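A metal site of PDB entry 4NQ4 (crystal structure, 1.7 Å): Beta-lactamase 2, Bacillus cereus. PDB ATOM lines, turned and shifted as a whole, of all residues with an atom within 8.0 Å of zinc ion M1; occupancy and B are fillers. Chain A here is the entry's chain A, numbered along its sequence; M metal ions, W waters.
The side-chain carboxylate of Asp 85 is in salt-bridge range of the guanidinium group of Arg 86 (3.9 Å). N of His 144 sits at hydrogen-bond distance from OD1 of Asn 148 (2.8 Å). NE2 of His 83 sits at hydrogen-bond distance from OD2 of Asp 178.
Asp 85 touches zinc ion M1 (OD1 to ZN, 3.9 Å). Within 4 Å of zinc ion M1: His 81, His 83, Asp 85 and His 144. Along chain A the residues within 4 Å of zinc ion M1 span positions 81 to 144. The nearest printed residue that does not touch zinc ion M1 is Cys 163 (4.04 Å).
Zinc ion M1 is bound by a ring nitrogen (ND1) of His 83 (2.0 Å), a ring nitrogen (NE2) of His 144 (2.0 Å), a ring nitrogen (NE2) of His 81 (2.1 Å) and water W1 (2.3 Å).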
ATOM      1  N   TRP A  54     -20.858  -3.873  10.845  1.00  0.00           N
ATOM      2  CA  TRP A  54     -20.765  -5.111  11.613  1.00  0.00           C
ATOM      3  C   TRP A  54     -20.317  -6.399  10.916  1.00  0.00           C
ATOM      4  O   TRP A  54     -19.613  -7.213  11.511  1.00  0.00           O
ATOM      5  CB  TRP A  54     -22.119  -5.354  12.312  1.00  0.00           C
ATOM      6  CG  TRP A  54     -22.529  -4.326  13.262  1.00  0.00           C
ATOM      7  CD1 TRP A  54     -23.472  -3.352  13.088  1.00  0.00           C
ATOM      8  CD2 TRP A  54     -22.068  -4.214  14.590  1.00  0.00           C
ATOM      9  NE1 TRP A  54     -23.609  -2.589  14.238  1.00  0.00           N
ATOM     10  CE2 TRP A  54     -22.754  -3.112  15.188  1.00  0.00           C
ATOM     11  CE3 TRP A  54     -21.110  -4.912  15.349  1.00  0.00           C
ATOM     12  CZ2 TRP A  54     -22.490  -2.681  16.484  1.00  0.00           C
ATOM     13  CZ3 TRP A  54     -20.871  -4.508  16.666  1.00  0.00           C
ATOM     14  CH2 TRP A  54     -21.585  -3.397  17.222  1.00  0.00           C
ATOM     15  N   THR A  80     -11.503   3.091  11.016  1.00  0.00           N
ATOM     16  CA  THR A  80     -11.085   3.906  12.140  1.00  0.00           C
ATOM     17  C   THR A  80     -10.620   3.159  13.415  1.00  0.00           C
ATOM     18  O   THR A  80      -9.926   3.734  14.241  1.00  0.00           O
ATOM     19  CB  THR A  80     -12.144   4.947  12.556  1.00  0.00           C
ATOM     20  OG1 THR A  80     -13.326   4.291  13.016  1.00  0.00           O
ATOM     21  CG2 THR A  80     -12.397   5.902  11.348  1.00  0.00           C
ATOM     22  N   HIS A  81     -10.869   1.868  13.422  1.00  0.00           N
ATOM     23  CA  HIS A  81     -10.193   0.876  14.307  1.00  0.00           C
ATOM     24  C   HIS A  81     -10.619  -0.579  13.944  1.00  0.00           C
ATOM     25  O   HIS A  81     -11.555  -0.782  13.210  1.00  0.00           O
ATOM     26  CB  HIS A  81     -10.308   1.150  15.837  1.00  0.00           C
ATOM     27  CG  HIS A  81     -11.674   0.993  16.403  1.00  0.00           C
ATOM     28  ND1 HIS A  81     -12.631   1.967  16.335  1.00  0.00           N
ATOM     29  CD2 HIS A  81     -12.257  -0.051  17.046  1.00  0.00           C
ATOM     30  CE1 HIS A  81     -13.731   1.549  16.915  1.00  0.00           C
ATOM     31  NE2 HIS A  81     -13.533   0.327  17.369  1.00  0.00           N
ATOM     32  N   ALA A  82      -9.944  -1.566  14.520  1.00  0.00           N
ATOM     33  CA  ALA A  82     -10.107  -2.998  14.190  1.00  0.00           C
ATOM     34  C   ALA A  82     -11.186  -3.810  14.992  1.00  0.00           C
ATOM     35  O   ALA A  82     -10.978  -5.000  15.222  1.00  0.00           O
ATOM     36  CB  ALA A  82      -8.734  -3.685  14.368  1.00  0.00           C
ATOM     37  N   HIS A  83     -12.310  -3.234  15.421  1.00  0.00           N
ATOM     38  CA  HIS A  83     -13.446  -3.947  15.978  1.00  0.00           C
ATOM     39  C   HIS A  83     -14.462  -4.200  14.848  1.00  0.00           C
ATOM     40  O   HIS A  83     -14.485  -3.452  13.852  1.00  0.00           O
ATOM     41  CB  HIS A  83     -14.169  -3.095  17.077  1.00  0.00           C
ATOM     42  CG  HIS A  83     -13.442  -3.090  18.384  1.00  0.00           C
ATOM     43  ND1 HIS A  83     -13.675  -2.140  19.369  1.00  0.00           N
ATOM     44  CD2 HIS A  83     -12.550  -3.956  18.910  1.00  0.00           C
ATOM     45  CE1 HIS A  83     -12.960  -2.432  20.432  1.00  0.00           C
ATOM     46  NE2 HIS A  83     -12.289  -3.538  20.195  1.00  0.00           N
ATOM     47  N   ALA A  84     -15.323  -5.209  15.036  1.00  0.00           N
ATOM     48  CA  ALA A  84     -16.198  -5.662  13.960  1.00  0.00           C
ATOM     49  C   ALA A  84     -17.144  -4.599  13.417  1.00  0.00           C
ATOM     50  O   ALA A  84     -17.579  -4.754  12.317  1.00  0.00           O
ATOM     51  CB  ALA A  84     -17.014  -6.877  14.381  1.00  0.00           C
ATOM     52  N   ASP A  85     -17.539  -3.610  14.214  1.00  0.00           N
ATOM     53  CA  ASP A  85     -18.467  -2.590  13.748  1.00  0.00           C
ATOM     54  C   ASP A  85     -17.894  -1.601  12.741  1.00  0.00           C
ATOM     55  O   ASP A  85     -18.616  -0.910  12.015  1.00  0.00           O
ATOM     56  CB  ASP A  85     -19.033  -1.816  14.923  1.00  0.00           C
ATOM     57  CG  ASP A  85     -17.997  -1.061  15.732  1.00  0.00           C
ATOM     58  OD1 ASP A  85     -17.015  -1.669  16.197  1.00  0.00           O
ATOM     59  OD2 ASP A  85     -18.317   0.120  16.008  1.00  0.00           O
ATOM     60  N   ARG A  86     -16.566  -1.547  12.708  1.00  0.00           N
ATOM     61  CA  ARG A  86     -15.796  -0.693  11.811  1.00  0.00           C
ATOM     62  C   ARG A  86     -15.322  -1.513  10.643  1.00  0.00           C
ATOM     63  O   ARG A  86     -15.386  -1.034   9.518  1.00  0.00           O
ATOM     64  CB  ARG A  86     -14.503  -0.205  12.493  1.00  0.00           C
ATOM     65  CG  ARG A  86     -14.645   0.528  13.843  1.00  0.00           C
ATOM     66  CD  ARG A  86     -15.478   1.806  13.735  1.00  0.00           C
ATOM     67  NE  ARG A  86     -16.847   1.728  14.218  1.00  0.00           N
ATOM     68  CZ  ARG A  86     -17.794   2.645  13.965  1.00  0.00           C
ATOM     69  NH1 ARG A  86     -18.996   2.504  14.466  1.00  0.00           N
ATOM     70  NH2 ARG A  86     -17.569   3.700  13.215  1.00  0.00           N
ATOM     71  N   HIS A 144     -10.462   4.427  23.374  1.00  0.00           N
ATOM     72  CA  HIS A 144     -11.394   3.298  23.213  1.00  0.00           C
ATOM     73  C   HIS A 144     -10.697   1.999  22.797  1.00  0.00           C
ATOM     74  O   HIS A 144     -10.978   0.953  23.343  1.00  0.00           O
ATOM     75  CB  HIS A 144     -12.496   3.688  22.194  1.00  0.00           C
ATOM     76  CG  HIS A 144     -13.287   2.535  21.667  1.00  0.00           C
ATOM     77  ND1 HIS A 144     -14.234   1.878  22.415  1.00  0.00           N
ATOM     78  CD2 HIS A 144     -13.223   1.876  20.480  1.00  0.00           C
ATOM     79  CE1 HIS A 144     -14.762   0.901  21.698  1.00  0.00           C
ATOM     80  NE2 HIS A 144     -14.176   0.894  20.526  1.00  0.00           N
ATOM     81  N   THR A 145      -9.796   2.119  21.806  1.00  0.00           N
ATOM     82  CA  THR A 145      -8.784   1.123  21.526  1.00  0.00           C
ATOM     83  C   THR A 145      -7.400   1.740  21.356  1.00  0.00           C
ATOM     84  O   THR A 145      -7.185   2.988  21.329  1.00  0.00           O
ATOM     85  CB  THR A 145      -9.126   0.442  20.219  1.00  0.00           C
ATOM     86  OG1 THR A 145      -9.165   1.407  19.188  1.00  0.00           O
ATOM     87  CG2 THR A 145     -10.470  -0.333  20.372  1.00  0.00           C
ATOM     88  N   ASP A 147      -5.580   1.749  18.621  1.00  0.00           N
ATOM     89  CA  ASP A 147      -5.392   2.291  17.281  1.00  0.00           C
ATOM     90  C   ASP A 147      -6.376   3.367  16.778  1.00  0.00           C
ATOM     91  O   ASP A 147      -6.247   3.862  15.619  1.00  0.00           O
ATOM     92  CB  ASP A 147      -5.482   1.104  16.335  1.00  0.00           C
ATOM     93  CG  ASP A 147      -6.784   0.363  16.404  1.00  0.00           C
ATOM     94  OD1 ASP A 147      -7.393   0.145  17.518  1.00  0.00           O
ATOM     95  OD2 ASP A 147      -7.242   0.003  15.325  1.00  0.00           O
ATOM     96  N   ASN A 148      -7.406   3.631  17.599  1.00  0.00           N
ATOM     97  CA  ASN A 148      -8.508   4.472  17.171  1.00  0.00           C
ATOM     98  C   ASN A 148      -8.053   5.820  16.573  1.00  0.00           C
ATOM     99  O   ASN A 148      -7.232   6.541  17.159  1.00  0.00           O
ATOM    100  CB  ASN A 148      -9.573   4.625  18.322  1.00  0.00           C
ATOM    101  CG  ASN A 148      -9.058   5.274  19.689  1.00  0.00           C
ATOM    102  OD1 ASN A 148      -9.759   5.066  20.692  1.00  0.00           O
ATOM    103  ND2 ASN A 148      -7.979   5.989  19.723  1.00  0.00           N
ATOM    104  N   GLY A 162     -15.845   8.576  15.904  1.00  0.00           N
ATOM    105  CA  GLY A 162     -15.781   7.147  16.032  1.00  0.00           C
ATOM    106  C   GLY A 162     -16.009   6.711  17.474  1.00  0.00           C
ATOM    107  O   GLY A 162     -16.583   7.428  18.240  1.00  0.00           O
ATOM    108  N   CYS A 163     -15.500   5.539  17.818  1.00  0.00           N
ATOM    109  CA  CYS A 163     -15.853   4.908  19.097  1.00  0.00           C
ATOM    110  C   CYS A 163     -15.014   5.480  20.286  1.00  0.00           C
ATOM    111  O   CYS A 163     -15.254   5.147  21.430  1.00  0.00           O
ATOM    112  CB  CYS A 163     -15.804   3.412  18.896  1.00  0.00           C
ATOM    113  SG  CYS A 163     -16.834   2.996  17.463  1.00  0.00           S
ATOM    114  N   LEU A 164     -14.024   6.296  19.958  1.00  0.00           N
ATOM    115  CA  LEU A 164     -13.307   7.221  20.882  1.00  0.00           C
ATOM    116  C   LEU A 164     -14.300   8.188  21.517  1.00  0.00           C
ATOM    117  O   LEU A 164     -14.094   8.567  22.704  1.00  0.00           O
ATOM    118  CB  LEU A 164     -12.202   8.003  20.178  1.00  0.00           C
ATOM    119  CG  LEU A 164     -11.298   8.916  20.991  1.00  0.00           C
ATOM    120  CD1 LEU A 164     -10.282   8.094  21.815  1.00  0.00           C
ATOM    121  CD2 LEU A 164     -10.641   9.782  19.938  1.00  0.00           C
ATOM    122  N   LYS A 166     -18.097   9.160  22.893  1.00  0.00           N
ATOM    123  CA  LYS A 166     -19.361   8.612  23.399  1.00  0.00           C
ATOM    124  C   LYS A 166     -20.458   9.635  23.145  1.00  0.00           C
ATOM    125  O   LYS A 166     -20.230  10.866  23.278  1.00  0.00           O
ATOM    126  CB  LYS A 166     -19.255   8.323  24.914  1.00  0.00           C
ATOM    127  CG  LYS A 166     -18.095   7.435  25.367  1.00  0.00           C
ATOM    128  CD  LYS A 166     -17.996   6.191  24.472  1.00  0.00           C
ATOM    129  CE  LYS A 166     -19.079   5.143  24.675  1.00  0.00           C
ATOM    130  NZ  LYS A 166     -18.518   3.782  24.508  1.00  0.00           N
ATOM    131  N   ASN A 175     -17.655  -1.291  26.433  1.00  0.00           N
ATOM    132  CA  ASN A 175     -16.645  -2.336  26.472  1.00  0.00           C
ATOM    133  C   ASN A 175     -15.244  -1.712  26.460  1.00  0.00           C
ATOM    134  O   ASN A 175     -14.892  -1.053  25.515  1.00  0.00           O
ATOM    135  CB  ASN A 175     -16.810  -3.320  25.296  1.00  0.00           C
ATOM    136  CG  ASN A 175     -16.290  -4.717  25.622  1.00  0.00           C
ATOM    137  OD1 ASN A 175     -17.023  -5.701  25.498  1.00  0.00           O
ATOM    138  ND2 ASN A 175     -15.041  -4.818  26.014  1.00  0.00           N
ATOM    139  N   ASP A 178     -10.438  -3.671  25.381  1.00  0.00           N
ATOM    140  CA  ASP A 178      -9.402  -3.224  24.467  1.00  0.00           C
ATOM    141  C   ASP A 178      -8.977  -1.777  24.708  1.00  0.00           C
ATOM    142  O   ASP A 178      -8.221  -1.222  23.921  1.00  0.00           O
ATOM    143  CB  ASP A 178      -9.904  -3.513  23.026  1.00  0.00           C
ATOM    144  CG  ASP A 178      -9.952  -4.980  22.729  1.00  0.00           C
ATOM    145  OD1 ASP A 178      -9.217  -5.771  23.399  1.00  0.00           O
ATOM    146  OD2 ASP A 178     -10.720  -5.393  21.848  1.00  0.00           O
ATOM    147  N   HIS A 205     -21.414   5.387  17.997  1.00  0.00           N
ATOM    148  CA  HIS A 205     -22.707   4.853  18.341  1.00  0.00           C
ATOM    149  C   HIS A 205     -23.506   5.966  19.003  1.00  0.00           C
ATOM    150  O   HIS A 205     -23.023   6.599  19.954  1.00  0.00           O
ATOM    151  CB  HIS A 205     -22.577   3.715  19.340  1.00  0.00           C
ATOM    152  CG  HIS A 205     -21.549   2.704  18.952  1.00  0.00           C
ATOM    153  ND1 HIS A 205     -21.842   1.616  18.162  1.00  0.00           N
ATOM    154  CD2 HIS A 205     -20.243   2.613  19.251  1.00  0.00           C
ATOM    155  CE1 HIS A 205     -20.731   0.931  17.942  1.00  0.00           C
ATOM    156  NE2 HIS A 205     -19.766   1.482  18.650  1.00  0.00           N
HETATM  157 ZN    ZN M   1     -14.585  -0.440  19.046  1.00  0.00          ZN
HETATM  158 ZN    ZN M   2     -17.871   0.970  17.973  1.00  0.00          ZN
HETATM  159  O   HOH W   1     -16.855  -0.442  19.304  1.00  0.00           O
